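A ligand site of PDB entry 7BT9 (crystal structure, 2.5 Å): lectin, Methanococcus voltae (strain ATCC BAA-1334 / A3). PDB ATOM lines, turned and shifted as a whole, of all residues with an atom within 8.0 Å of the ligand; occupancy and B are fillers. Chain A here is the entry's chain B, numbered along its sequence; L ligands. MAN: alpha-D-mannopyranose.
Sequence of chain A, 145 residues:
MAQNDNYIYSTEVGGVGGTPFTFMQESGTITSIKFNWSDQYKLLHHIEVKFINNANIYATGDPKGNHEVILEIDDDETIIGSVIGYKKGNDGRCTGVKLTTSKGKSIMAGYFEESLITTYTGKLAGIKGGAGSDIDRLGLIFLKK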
ATOM      1  N   GLY A  15       1.589 -19.376  29.684  1.00  0.00           N
ATOM      2  CA  GLY A  15       0.562 -20.228  30.318  1.00  0.00           C
ATOM      3  C   GLY A  15      -0.174 -21.097  29.304  1.00  0.00           C
ATOM      4  O   GLY A  15       0.131 -21.025  28.057  1.00  0.00           O
ATOM      5  N   VAL A  16      -1.157 -21.840  29.835  1.00  0.00           N
ATOM      6  CA  VAL A  16      -2.062 -22.746  29.061  1.00  0.00           C
ATOM      7  C   VAL A  16      -3.305 -21.987  28.558  1.00  0.00           C
ATOM      8  O   VAL A  16      -4.036 -22.604  27.728  1.00  0.00           O
ATOM      9  CB  VAL A  16      -2.441 -23.993  29.873  1.00  0.00           C
ATOM     10  CG1 VAL A  16      -1.211 -24.811  30.228  1.00  0.00           C
ATOM     11  CG2 VAL A  16      -3.228 -23.650  31.127  1.00  0.00           C
ATOM     12  N   GLY A  17      -3.501 -20.722  28.969  1.00  0.00           N
ATOM     13  CA  GLY A  17      -4.706 -19.915  28.699  1.00  0.00           C
ATOM     14  C   GLY A  17      -4.895 -19.555  27.239  1.00  0.00           C
ATOM     15  O   GLY A  17      -4.030 -19.890  26.355  1.00  0.00           O
ATOM     16  N   GLY A  18      -6.025 -18.918  26.950  1.00  0.00           N
ATOM     17  CA  GLY A  18      -6.256 -18.233  25.668  1.00  0.00           C
ATOM     18  C   GLY A  18      -6.578 -19.156  24.517  1.00  0.00           C
ATOM     19  O   GLY A  18      -6.438 -20.366  24.624  1.00  0.00           O
ATOM     20  N   THR A  19      -6.986 -18.565  23.419  1.00  0.00           N
ATOM     21  CA  THR A  19      -7.346 -19.255  22.158  1.00  0.00           C
ATOM     22  C   THR A  19      -6.067 -19.634  21.415  1.00  0.00           C
ATOM     23  O   THR A  19      -5.291 -18.741  21.136  1.00  0.00           O
ATOM     24  CB  THR A  19      -8.221 -18.297  21.339  1.00  0.00           C
ATOM     25  OG1 THR A  19      -9.498 -18.260  21.974  1.00  0.00           O
ATOM     26  CG2 THR A  19      -8.388 -18.713  19.901  1.00  0.00           C
ATOM     27  N   PRO A  20      -5.827 -20.914  21.008  1.00  0.00           N
ATOM     28  CA  PRO A  20      -4.716 -21.240  20.109  1.00  0.00           C
ATOM     29  C   PRO A  20      -4.655 -20.414  18.812  1.00  0.00           C
ATOM     30  O   PRO A  20      -5.708 -20.092  18.238  1.00  0.00           O
ATOM     31  CB  PRO A  20      -4.916 -22.729  19.769  1.00  0.00           C
ATOM     32  CG  PRO A  20      -5.582 -23.238  21.014  1.00  0.00           C
ATOM     33  CD  PRO A  20      -6.549 -22.126  21.422  1.00  0.00           C
ATOM     34  N   LEU A  43       2.087  -6.567  30.320  1.00  0.00           N
ATOM     35  CA  LEU A  43       1.923  -7.810  29.523  1.00  0.00           C
ATOM     36  C   LEU A  43       1.889  -7.466  28.046  1.00  0.00           C
ATOM     37  O   LEU A  43       1.388  -6.417  27.739  1.00  0.00           O
ATOM     38  CB  LEU A  43       0.598  -8.471  29.911  1.00  0.00           C
ATOM     39  CG  LEU A  43       0.450  -8.880  31.368  1.00  0.00           C
ATOM     40  CD1 LEU A  43      -0.946  -9.438  31.639  1.00  0.00           C
ATOM     41  CD2 LEU A  43       1.492  -9.909  31.758  1.00  0.00           C
ATOM     42  N   LEU A  44       2.326  -8.378  27.181  1.00  0.00           N
ATOM     43  CA  LEU A  44       1.866  -8.379  25.776  1.00  0.00           C
ATOM     44  C   LEU A  44       0.402  -8.803  25.757  1.00  0.00           C
ATOM     45  O   LEU A  44       0.001  -9.750  26.489  1.00  0.00           O
ATOM     46  CB  LEU A  44       2.689  -9.377  24.962  1.00  0.00           C
ATOM     47  CG  LEU A  44       4.197  -9.311  25.112  1.00  0.00           C
ATOM     48  CD1 LEU A  44       4.849 -10.226  24.081  1.00  0.00           C
ATOM     49  CD2 LEU A  44       4.681  -7.898  24.915  1.00  0.00           C
ATOM     50  N   HIS A  45      -0.355  -8.136  24.891  1.00  0.00           N
ATOM     51  CA  HIS A  45      -1.820  -8.322  24.713  1.00  0.00           C
ATOM     52  C   HIS A  45      -2.128  -8.818  23.309  1.00  0.00           C
ATOM     53  O   HIS A  45      -2.996  -9.718  23.211  1.00  0.00           O
ATOM     54  CB  HIS A  45      -2.543  -6.997  24.943  1.00  0.00           C
ATOM     55  CG  HIS A  45      -2.511  -6.590  26.361  1.00  0.00           C
ATOM     56  ND1 HIS A  45      -3.205  -7.287  27.315  1.00  0.00           N
ATOM     57  CD2 HIS A  45      -1.861  -5.587  26.985  1.00  0.00           C
ATOM     58  CE1 HIS A  45      -2.995  -6.727  28.484  1.00  0.00           C
ATOM     59  NE2 HIS A  45      -2.186  -5.672  28.309  1.00  0.00           N
ATOM     60  N   GLY A  61      -5.077 -11.985  19.978  1.00  0.00           N
ATOM     61  CA  GLY A  61      -5.079 -11.133  21.174  1.00  0.00           C
ATOM     62  C   GLY A  61      -5.937  -9.899  21.062  1.00  0.00           C
ATOM     63  O   GLY A  61      -6.346  -9.549  19.994  1.00  0.00           O
ATOM     64  N   ASP A  62      -6.174  -9.270  22.200  1.00  0.00           N
ATOM     65  CA  ASP A  62      -6.976  -8.036  22.336  1.00  0.00           C
ATOM     66  C   ASP A  62      -6.025  -6.842  22.267  1.00  0.00           C
ATOM     67  O   ASP A  62      -5.234  -6.679  23.181  1.00  0.00           O
ATOM     68  CB  ASP A  62      -7.812  -8.117  23.615  1.00  0.00           C
ATOM     69  CG  ASP A  62      -8.704  -6.921  23.862  1.00  0.00           C
ATOM     70  OD1 ASP A  62      -8.915  -6.171  22.936  1.00  0.00           O
ATOM     71  OD2 ASP A  62      -9.145  -6.770  24.985  1.00  0.00           O
ATOM     72  N   LYS A  64      -5.300  -3.925  23.328  1.00  0.00           N
ATOM     73  CA  LYS A  64      -5.716  -2.952  24.371  1.00  0.00           C
ATOM     74  C   LYS A  64      -4.499  -2.280  25.039  1.00  0.00           C
ATOM     75  O   LYS A  64      -4.678  -1.438  25.909  1.00  0.00           O
ATOM     76  CB  LYS A  64      -6.642  -3.644  25.363  1.00  0.00           C
ATOM     77  CG  LYS A  64      -6.042  -4.667  26.298  1.00  0.00           C
ATOM     78  CD  LYS A  64      -7.073  -5.122  27.289  1.00  0.00           C
ATOM     79  CE  LYS A  64      -6.528  -5.948  28.417  1.00  0.00           C
ATOM     80  NZ  LYS A  64      -7.578  -6.847  28.953  1.00  0.00           N
ATOM     81  N   ASN A  90       1.084 -22.546  34.824  1.00  0.00           N
ATOM     82  CA  ASN A  90      -0.185 -22.738  34.046  1.00  0.00           C
ATOM     83  C   ASN A  90      -0.939 -21.419  33.864  1.00  0.00           C
ATOM     84  O   ASN A  90      -1.484 -21.227  32.794  1.00  0.00           O
ATOM     85  CB  ASN A  90      -1.106 -23.791  34.671  1.00  0.00           C
ATOM     86  CG  ASN A  90      -0.472 -25.163  34.636  1.00  0.00           C
ATOM     87  OD1 ASN A  90       0.054 -25.566  33.605  1.00  0.00           O
ATOM     88  ND2 ASN A  90      -0.451 -25.840  35.770  1.00  0.00           N
ATOM     89  N   ASP A  91      -0.963 -20.552  34.870  1.00  0.00           N
ATOM     90  CA  ASP A  91      -1.709 -19.273  34.783  1.00  0.00           C
ATOM     91  C   ASP A  91      -0.745 -18.199  34.216  1.00  0.00           C
ATOM     92  O   ASP A  91      -0.984 -16.993  34.387  1.00  0.00           O
ATOM     93  CB  ASP A  91      -2.367 -19.010  36.141  1.00  0.00           C
ATOM     94  CG  ASP A  91      -3.465 -17.962  36.074  1.00  0.00           C
ATOM     95  OD1 ASP A  91      -3.912 -17.639  34.939  1.00  0.00           O
ATOM     96  OD2 ASP A  91      -3.830 -17.444  37.158  1.00  0.00           O
ATOM     97  N   GLY A  92       0.269 -18.632  33.484  1.00  0.00           N
ATOM     98  CA  GLY A  92       1.385 -17.772  33.056  1.00  0.00           C
ATOM     99  C   GLY A  92       1.021 -16.889  31.876  1.00  0.00           C
ATOM    100  O   GLY A  92      -0.073 -17.077  31.310  1.00  0.00           O
ATOM    101  N   ARG A  93       1.901 -15.947  31.538  1.00  0.00           N
ATOM    102  CA  ARG A  93       1.677 -14.960  30.460  1.00  0.00           C
ATOM    103  C   ARG A  93       2.994 -14.520  29.814  1.00  0.00           C
ATOM    104  O   ARG A  93       4.008 -14.621  30.455  1.00  0.00           O
ATOM    105  CB  ARG A  93       1.159 -13.633  31.024  1.00  0.00           C
ATOM    106  CG  ARG A  93      -0.236 -13.649  31.596  1.00  0.00           C
ATOM    107  CD  ARG A  93      -1.275 -14.163  30.639  1.00  0.00           C
ATOM    108  NE  ARG A  93      -2.569 -13.793  31.160  1.00  0.00           N
ATOM    109  CZ  ARG A  93      -3.246 -14.472  32.045  1.00  0.00           C
ATOM    110  NH1 ARG A  93      -2.774 -15.587  32.537  1.00  0.00           N
ATOM    111  NH2 ARG A  93      -4.412 -14.029  32.424  1.00  0.00           N
ATOM    112  N   GLY A 130      -1.119 -19.152  22.426  1.00  0.00           N
ATOM    113  CA  GLY A 130      -2.499 -18.855  22.799  1.00  0.00           C
ATOM    114  C   GLY A 130      -2.631 -17.466  23.380  1.00  0.00           C
ATOM    115  O   GLY A 130      -1.742 -17.049  24.108  1.00  0.00           O
ATOM    116  N   ALA A 131      -3.740 -16.806  23.085  1.00  0.00           N
ATOM    117  CA  ALA A 131      -4.029 -15.385  23.386  1.00  0.00           C
ATOM    118  C   ALA A 131      -5.535 -15.186  23.528  1.00  0.00           C
ATOM    119  O   ALA A 131      -6.295 -15.818  22.747  1.00  0.00           O
ATOM    120  CB  ALA A 131      -3.481 -14.504  22.304  1.00  0.00           C
ATOM    121  N   GLY A 132      -5.918 -14.370  24.511  1.00  0.00           N
ATOM    122  CA  GLY A 132      -7.278 -13.806  24.663  1.00  0.00           C
ATOM    123  C   GLY A 132      -7.177 -12.325  24.946  1.00  0.00           C
ATOM    124  O   GLY A 132      -6.776 -11.604  24.055  1.00  0.00           O
ATOM    125  N   SER A 133      -7.502 -11.879  26.151  1.00  0.00           N
ATOM    126  CA  SER A 133      -7.211 -10.508  26.626  1.00  0.00           C
ATOM    127  C   SER A 133      -5.721 -10.199  26.476  1.00  0.00           C
ATOM    128  O   SER A 133      -5.367  -9.042  26.230  1.00  0.00           O
ATOM    129  CB  SER A 133      -7.614 -10.336  28.079  1.00  0.00           C
ATOM    130  OG  SER A 133      -8.990 -10.055  28.165  1.00  0.00           O
ATOM    131  N   ASP A 134      -4.888 -11.206  26.749  1.00  0.00           N
ATOM    132  CA  ASP A 134      -3.407 -11.160  26.769  1.00  0.00           C
ATOM    133  C   ASP A 134      -2.829 -12.186  25.776  1.00  0.00           C
ATOM    134  O   ASP A 134      -3.593 -12.995  25.175  1.00  0.00           O
ATOM    135  CB  ASP A 134      -2.915 -11.486  28.173  1.00  0.00           C
ATOM    136  CG  ASP A 134      -3.599 -10.674  29.244  1.00  0.00           C
ATOM    137  OD1 ASP A 134      -4.140  -9.596  28.897  1.00  0.00           O
ATOM    138  OD2 ASP A 134      -3.565 -11.117  30.411  1.00  0.00           O
ATOM    139  N   ILE A 135      -1.506 -12.156  25.626  1.00  0.00           N
ATOM    140  CA  ILE A 135      -0.733 -13.262  25.027  1.00  0.00           C
ATOM    141  C   ILE A 135      -0.405 -14.200  26.188  1.00  0.00           C
ATOM    142  O   ILE A 135       0.419 -13.841  27.052  1.00  0.00           O
ATOM    143  CB  ILE A 135       0.517 -12.731  24.313  1.00  0.00           C
ATOM    144  CG1 ILE A 135       0.163 -11.574  23.384  1.00  0.00           C
ATOM    145  CG2 ILE A 135       1.262 -13.858  23.599  1.00  0.00           C
ATOM    146  CD1 ILE A 135      -0.727 -11.986  22.237  1.00  0.00           C
ATOM    147  N   ASP A 136      -1.087 -15.332  26.282  1.00  0.00           N
ATOM    148  CA  ASP A 136      -0.789 -16.308  27.375  1.00  0.00           C
ATOM    149  C   ASP A 136       0.565 -16.958  27.056  1.00  0.00           C
ATOM    150  O   ASP A 136       1.361 -17.098  27.980  1.00  0.00           O
ATOM    151  CB  ASP A 136      -1.907 -17.325  27.543  1.00  0.00           C
ATOM    152  CG  ASP A 136      -3.241 -16.671  27.869  1.00  0.00           C
ATOM    153  OD1 ASP A 136      -3.902 -16.125  26.911  1.00  0.00           O
ATOM    154  OD2 ASP A 136      -3.589 -16.693  29.100  1.00  0.00           O
ATOM    155  N   ARG A 137       0.828 -17.205  25.768  1.00  0.00           N
ATOM    156  CA  ARG A 137       1.811 -18.208  25.307  1.00  0.00           C
ATOM    157  C   ARG A 137       2.331 -17.828  23.921  1.00  0.00           C
ATOM    158  O   ARG A 137       1.513 -17.457  23.080  1.00  0.00           O
ATOM    159  CB  ARG A 137       1.074 -19.544  25.316  1.00  0.00           C
ATOM    160  CG  ARG A 137       1.970 -20.750  25.104  1.00  0.00           C
ATOM    161  CD  ARG A 137       1.242 -22.064  25.336  1.00  0.00           C
ATOM    162  NE  ARG A 137       0.152 -22.315  24.386  1.00  0.00           N
ATOM    163  CZ  ARG A 137      -1.143 -22.198  24.660  1.00  0.00           C
ATOM    164  NH1 ARG A 137      -1.563 -21.769  25.842  1.00  0.00           N
ATOM    165  NH2 ARG A 137      -2.025 -22.477  23.726  1.00  0.00           N
HETATM  166  C1  MAN L   1      -9.197 -14.555  27.671  1.00  0.00           C
HETATM  167  C2  MAN L   1      -9.288 -16.049  27.543  1.00  0.00           C
HETATM  168  C3  MAN L   1      -8.531 -16.776  28.631  1.00  0.00           C
HETATM  169  C4  MAN L   1      -7.136 -16.205  28.830  1.00  0.00           C
HETATM  170  C5  MAN L   1      -7.242 -14.720  29.165  1.00  0.00           C
HETATM  171  C6  MAN L   1      -5.882 -14.073  29.310  1.00  0.00           C
HETATM  172  O1  MAN L   1     -10.140 -14.261  28.687  1.00  0.00           O
HETATM  173  O2  MAN L   1      -8.821 -16.505  26.273  1.00  0.00           O
HETATM  174  O3  MAN L   1      -8.514 -18.132  28.218  1.00  0.00           O
HETATM  175  O4  MAN L   1      -6.437 -16.943  29.831  1.00  0.00           O
HETATM  176  O5  MAN L   1      -7.900 -14.053  28.049  1.00  0.00           O
HETATM  177  O6  MAN L   1      -5.368 -13.745  27.982  1.00  0.00           O
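The side-chain carboxylate (OD2) of Asp 134 is in salt-bridge range of the guanidinium group (NE) of Arg 93.
The side-chain carboxylate (OD1) of Asp 134 is in hydrogen-bond range of a ring nitrogen (ND1) of His 45, 3.0 Å away.
The backbone carbonyl oxygen (O) of Ser 133 sits at hydrogen-bond distance from a ring nitrogen (ND1) of His 45, at 3.0 Å.
The side-chain carboxylate (OD2) of Asp 136 lies within salt-bridge range of the guanidinium group (NE) of Arg 93 (3.7 Å).
The backbone carbonyl oxygen (O) of Gly 130 lies within hydrogen-bond range of the backbone NH (N) of Asp 136.
O of Asp 136 sits at hydrogen-bond distance from N of Gly 15 (2.9 Å).
The guanidinium group of Arg 93 is in salt-bridge range of the side-chain carboxylate of Asp 91.
O of Ala 131 lies within hydrogen-bond range of N of Thr 19 (2.9 Å).
Merely in contact with the ligand: Gly 17 (3.6 Å), Thr 19 (3.97 Å), Arg 93 (3.4 Å) and Gly 132 (3.5 Å).
Of the 24 residues printed, 8 come within 4 Å of the ligand.
The nearest printed residue that does not touch the ligand is Ala 131 (4.4 Å).
An oxygen (O6) of the ligand sits at hydrogen-bond distance from the backbone NH (N) of Asp 134 (2.9 Å).
The backbone carbonyl oxygen of Asp 134 lies close to an oxygen (O6) of the ligand.
O3 of the ligand is in hydrogen-bond range of N of Gly 18.
O5 of the ligand lies within hydrogen-bond range of N of Ser 133, 2.9 Å away.
An oxygen (O4) of the ligand lies within hydrogen-bond range of the side-chain carboxylate (OD2) of Asp 136.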
